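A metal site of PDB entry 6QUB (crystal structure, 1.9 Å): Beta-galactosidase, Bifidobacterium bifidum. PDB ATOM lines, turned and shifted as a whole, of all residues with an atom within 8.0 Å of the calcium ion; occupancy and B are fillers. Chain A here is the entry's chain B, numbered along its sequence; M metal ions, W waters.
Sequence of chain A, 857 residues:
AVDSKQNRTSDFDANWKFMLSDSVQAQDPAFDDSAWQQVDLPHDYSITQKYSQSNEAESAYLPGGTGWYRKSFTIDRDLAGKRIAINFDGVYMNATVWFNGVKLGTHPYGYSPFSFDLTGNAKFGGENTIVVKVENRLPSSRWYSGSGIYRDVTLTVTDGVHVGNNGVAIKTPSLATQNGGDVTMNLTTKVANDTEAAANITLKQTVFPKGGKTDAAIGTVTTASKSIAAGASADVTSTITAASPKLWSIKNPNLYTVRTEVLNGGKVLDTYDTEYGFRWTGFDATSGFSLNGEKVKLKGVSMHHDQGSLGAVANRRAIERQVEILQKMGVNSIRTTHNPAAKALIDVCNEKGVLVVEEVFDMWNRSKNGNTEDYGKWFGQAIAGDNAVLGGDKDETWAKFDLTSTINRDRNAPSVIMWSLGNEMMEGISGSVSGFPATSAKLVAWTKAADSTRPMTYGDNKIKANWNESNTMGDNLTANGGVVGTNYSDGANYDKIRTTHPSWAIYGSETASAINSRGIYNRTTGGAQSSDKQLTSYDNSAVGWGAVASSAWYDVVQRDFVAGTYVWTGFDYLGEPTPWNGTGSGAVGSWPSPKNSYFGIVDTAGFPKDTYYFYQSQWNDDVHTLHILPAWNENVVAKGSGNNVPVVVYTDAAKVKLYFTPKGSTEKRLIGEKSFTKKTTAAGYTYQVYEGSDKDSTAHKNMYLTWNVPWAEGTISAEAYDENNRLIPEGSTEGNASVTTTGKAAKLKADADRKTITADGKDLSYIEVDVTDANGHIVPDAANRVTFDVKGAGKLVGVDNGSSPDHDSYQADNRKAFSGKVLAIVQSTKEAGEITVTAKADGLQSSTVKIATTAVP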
ATOM      1  N   TYR A 615      -5.413  -9.504  -8.837  1.00  0.00           N
ATOM      2  CA  TYR A 615      -5.008  -8.679  -9.978  1.00  0.00           C
ATOM      3  C   TYR A 615      -4.055  -7.587  -9.542  1.00  0.00           C
ATOM      4  O   TYR A 615      -3.068  -7.310 -10.236  1.00  0.00           O
ATOM      5  CB  TYR A 615      -6.230  -8.083 -10.660  1.00  0.00           C
ATOM      6  CG  TYR A 615      -6.946  -9.045 -11.595  1.00  0.00           C
ATOM      7  CD1 TYR A 615      -6.372  -9.435 -12.789  1.00  0.00           C
ATOM      8  CD2 TYR A 615      -8.179  -9.573 -11.256  1.00  0.00           C
ATOM      9  CE1 TYR A 615      -7.024 -10.316 -13.640  1.00  0.00           C
ATOM     10  CE2 TYR A 615      -8.834 -10.452 -12.098  1.00  0.00           C
ATOM     11  CZ  TYR A 615      -8.254 -10.829 -13.293  1.00  0.00           C
ATOM     12  OH  TYR A 615      -8.904 -11.702 -14.123  1.00  0.00           O
ATOM     13  N   GLN A 616      -4.331  -6.937  -8.416  1.00  0.00           N
ATOM     14  CA  GLN A 616      -3.431  -5.903  -7.930  1.00  0.00           C
ATOM     15  C   GLN A 616      -2.040  -6.459  -7.684  1.00  0.00           C
ATOM     16  O   GLN A 616      -1.043  -5.798  -7.998  1.00  0.00           O
ATOM     17  CB  GLN A 616      -3.972  -5.252  -6.651  1.00  0.00           C
ATOM     18  CG  GLN A 616      -3.173  -4.018  -6.213  1.00  0.00           C
ATOM     19  CD  GLN A 616      -3.618  -3.474  -4.871  1.00  0.00           C
ATOM     20  OE1 GLN A 616      -3.344  -4.076  -3.831  1.00  0.00           O
ATOM     21  NE2 GLN A 616      -4.315  -2.339  -4.885  1.00  0.00           N
ATOM     22  N   SER A 617      -1.959  -7.671  -7.129  1.00  0.00           N
ATOM     23  CA  SER A 617      -0.664  -8.303  -6.881  1.00  0.00           C
ATOM     24  C   SER A 617       0.059  -8.602  -8.182  1.00  0.00           C
ATOM     25  O   SER A 617       1.297  -8.663  -8.208  1.00  0.00           O
ATOM     26  CB  SER A 617      -0.845  -9.601  -6.090  1.00  0.00           C
ATOM     27  OG  SER A 617      -1.304 -10.654  -6.928  1.00  0.00           O
ATOM     28  N   GLN A 618      -0.683  -8.779  -9.283  1.00  0.00           N
ATOM     29  CA  GLN A 618      -0.116  -9.105 -10.589  1.00  0.00           C
ATOM     30  C   GLN A 618       0.214  -7.875 -11.418  1.00  0.00           C
ATOM     31  O   GLN A 618       1.129  -7.920 -12.242  1.00  0.00           O
ATOM     32  CB  GLN A 618      -1.095  -9.979 -11.374  1.00  0.00           C
ATOM     33  CG  GLN A 618      -1.430 -11.294 -10.704  1.00  0.00           C
ATOM     34  CD  GLN A 618      -0.183 -12.124 -10.430  1.00  0.00           C
ATOM     35  OE1 GLN A 618       0.486 -12.564 -11.361  1.00  0.00           O
ATOM     36  NE2 GLN A 618       0.140 -12.306  -9.162  1.00  0.00           N
ATOM     37  N   TRP A 619      -0.521  -6.784 -11.243  1.00  0.00           N
ATOM     38  CA  TRP A 619      -0.534  -5.701 -12.217  1.00  0.00           C
ATOM     39  C   TRP A 619       0.024  -4.393 -11.706  1.00  0.00           C
ATOM     40  O   TRP A 619       0.650  -3.658 -12.482  1.00  0.00           O
ATOM     41  CB  TRP A 619      -1.976  -5.484 -12.705  1.00  0.00           C
ATOM     42  CG  TRP A 619      -2.446  -6.528 -13.653  1.00  0.00           C
ATOM     43  CD1 TRP A 619      -1.726  -7.576 -14.154  1.00  0.00           C
ATOM     44  CD2 TRP A 619      -3.758  -6.647 -14.231  1.00  0.00           C
ATOM     45  NE1 TRP A 619      -2.494  -8.320 -15.007  1.00  0.00           N
ATOM     46  CE2 TRP A 619      -3.743  -7.771 -15.074  1.00  0.00           C
ATOM     47  CE3 TRP A 619      -4.933  -5.896 -14.109  1.00  0.00           C
ATOM     48  CZ2 TRP A 619      -4.867  -8.172 -15.803  1.00  0.00           C
ATOM     49  CZ3 TRP A 619      -6.046  -6.287 -14.847  1.00  0.00           C
ATOM     50  CH2 TRP A 619      -6.001  -7.419 -15.673  1.00  0.00           C
ATOM     51  N   ASN A 620      -0.188  -4.056 -10.435  1.00  0.00           N
ATOM     52  CA  ASN A 620       0.188  -2.736  -9.929  1.00  0.00           C
ATOM     53  C   ASN A 620       1.618  -2.774  -9.399  1.00  0.00           C
ATOM     54  O   ASN A 620       1.870  -3.255  -8.290  1.00  0.00           O
ATOM     55  CB  ASN A 620      -0.796  -2.276  -8.850  1.00  0.00           C
ATOM     56  CG  ASN A 620      -0.694  -0.798  -8.594  1.00  0.00           C
ATOM     57  OD1 ASN A 620       0.351  -0.193  -8.825  1.00  0.00           O
ATOM     58  ND2 ASN A 620      -1.793  -0.196  -8.143  1.00  0.00           N
ATOM     59  N   ASP A 621       2.552  -2.219 -10.164  1.00  0.00           N
ATOM     60  CA  ASP A 621       3.942  -2.152  -9.762  1.00  0.00           C
ATOM     61  C   ASP A 621       4.261  -0.954  -8.894  1.00  0.00           C
ATOM     62  O   ASP A 621       5.427  -0.770  -8.513  1.00  0.00           O
ATOM     63  CB  ASP A 621       4.849  -2.154 -11.000  1.00  0.00           C
ATOM     64  CG  ASP A 621       4.717  -3.429 -11.807  1.00  0.00           C
ATOM     65  OD1 ASP A 621       4.501  -4.497 -11.190  1.00  0.00           O
ATOM     66  OD2 ASP A 621       4.780  -3.349 -13.052  1.00  0.00           O
ATOM     67  N   ASP A 622       3.266  -0.124  -8.565  1.00  0.00           N
ATOM     68  CA  ASP A 622       3.469   1.056  -7.732  1.00  0.00           C
ATOM     69  C   ASP A 622       2.904   0.890  -6.336  1.00  0.00           C
ATOM     70  O   ASP A 622       2.917   1.841  -5.555  1.00  0.00           O
ATOM     71  CB  ASP A 622       2.840   2.286  -8.403  1.00  0.00           C
ATOM     72  CG  ASP A 622       3.530   2.661  -9.703  1.00  0.00           C
ATOM     73  OD1 ASP A 622       4.707   2.271  -9.886  1.00  0.00           O
ATOM     74  OD2 ASP A 622       2.897   3.343 -10.531  1.00  0.00           O
ATOM     75  N   VAL A 623       2.403  -0.306  -5.992  1.00  0.00           N
ATOM     76  CA  VAL A 623       1.877  -0.578  -4.660  1.00  0.00           C
ATOM     77  C   VAL A 623       2.212  -2.022  -4.308  1.00  0.00           C
ATOM     78  O   VAL A 623       2.486  -2.846  -5.180  1.00  0.00           O
ATOM     79  CB  VAL A 623       0.348  -0.344  -4.589  1.00  0.00           C
ATOM     80  CG1 VAL A 623      -0.410  -1.557  -5.106  1.00  0.00           C
ATOM     81  CG2 VAL A 623      -0.085   0.017  -3.187  1.00  0.00           C
ATOM     82  N   HIS A 624       2.218  -2.333  -3.021  1.00  0.00           N
ATOM     83  CA  HIS A 624       2.377  -3.708  -2.587  1.00  0.00           C
ATOM     84  C   HIS A 624       1.037  -4.268  -2.128  1.00  0.00           C
ATOM     85  O   HIS A 624       0.150  -3.535  -1.688  1.00  0.00           O
ATOM     86  CB  HIS A 624       3.420  -3.820  -1.470  1.00  0.00           C
ATOM     87  CG  HIS A 624       4.811  -3.449  -1.908  1.00  0.00           C
ATOM     88  ND1 HIS A 624       5.389  -3.977  -3.036  1.00  0.00           N
ATOM     89  CD2 HIS A 624       5.729  -2.609  -1.367  1.00  0.00           C
ATOM     90  CE1 HIS A 624       6.611  -3.482  -3.177  1.00  0.00           C
ATOM     91  NE2 HIS A 624       6.840  -2.650  -2.184  1.00  0.00           N
ATOM     92  N   THR A 625       0.881  -5.582  -2.275  1.00  0.00           N
ATOM     93  CA  THR A 625      -0.368  -6.249  -1.970  1.00  0.00           C
ATOM     94  C   THR A 625      -0.113  -7.393  -0.983  1.00  0.00           C
ATOM     95  O   THR A 625       0.878  -8.123  -1.115  1.00  0.00           O
ATOM     96  CB  THR A 625      -1.038  -6.798  -3.246  1.00  0.00           C
ATOM     97  OG1 THR A 625      -1.210  -5.730  -4.197  1.00  0.00           O
ATOM     98  CG2 THR A 625      -2.403  -7.399  -2.933  1.00  0.00           C
ATOM     99  N   THR A 651      -0.530 -11.780  -2.984  1.00  0.00           N
ATOM    100  CA  THR A 651       0.563 -10.883  -2.621  1.00  0.00           C
ATOM    101  C   THR A 651       1.535 -10.765  -3.786  1.00  0.00           C
ATOM    102  O   THR A 651       1.688 -11.704  -4.575  1.00  0.00           O
ATOM    103  CB  THR A 651       1.305 -11.372  -1.369  1.00  0.00           C
ATOM    104  OG1 THR A 651       2.258 -10.379  -0.961  1.00  0.00           O
ATOM    105  CG2 THR A 651       2.034 -12.684  -1.652  1.00  0.00           C
ATOM    106  N   ASP A 652       2.199  -9.615  -3.873  1.00  0.00           N
ATOM    107  CA  ASP A 652       3.335  -9.439  -4.765  1.00  0.00           C
ATOM    108  C   ASP A 652       4.660  -9.637  -4.052  1.00  0.00           C
ATOM    109  O   ASP A 652       5.715  -9.418  -4.652  1.00  0.00           O
ATOM    110  CB  ASP A 652       3.303  -8.064  -5.436  1.00  0.00           C
ATOM    111  CG  ASP A 652       3.490  -6.926  -4.450  1.00  0.00           C
ATOM    112  OD1 ASP A 652       3.091  -7.064  -3.272  1.00  0.00           O
ATOM    113  OD2 ASP A 652       4.036  -5.879  -4.866  1.00  0.00           O
ATOM    114  N   ALA A 653       4.630 -10.042  -2.787  1.00  0.00           N
ATOM    115  CA  ALA A 653       5.863 -10.269  -2.039  1.00  0.00           C
ATOM    116  C   ALA A 653       6.559 -11.539  -2.530  1.00  0.00           C
ATOM    117  O   ALA A 653       5.955 -12.442  -3.103  1.00  0.00           O
ATOM    118  CB  ALA A 653       5.568 -10.386  -0.535  1.00  0.00           C
HETATM  119 CA    CA M   1       3.071  -4.529  -6.701  1.00  0.00          CA
HETATM  120  O   HOH W   1       5.266  -3.515  -6.614  1.00  0.00           O
HETATM  121  O   HOH W   2       3.044  -6.221  -8.451  1.00  0.00           O
HETATM  122  O   HOH W   3       0.803  -5.495  -5.881  1.00  0.00           O
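OD1 of Asn 620 is in hydrogen-bond range of N of Asp 622 (2.9 Å).
The side-chain carboxylate (OD2) of Asp 652 sits close to a ring nitrogen (ND1) of His 624 (3.0 Å).
N of Thr 625 is in hydrogen-bond range of OD1 of Asp 652, 2.8 Å away.
Residues that only touch the calcium ion: Asp 621.
Of the 14 residues printed, 4 come within 4 Å of the calcium ion.
The calcium ion is bound by the backbone carbonyl oxygen (O) of Val 623, the backbone carbonyl oxygen (O) of Asn 620, water W1, water W2, the side-chain carboxylate (OD2) of Asp 652 and water W3.
The calcium ion has six donor atoms within binding distance.
Water W3 lies within hydrogen-bond range of the side-chain hydroxyl of Thr 625 (2.6 Å) and the backbone carbonyl oxygen of Gln 616 (2.8 Å).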
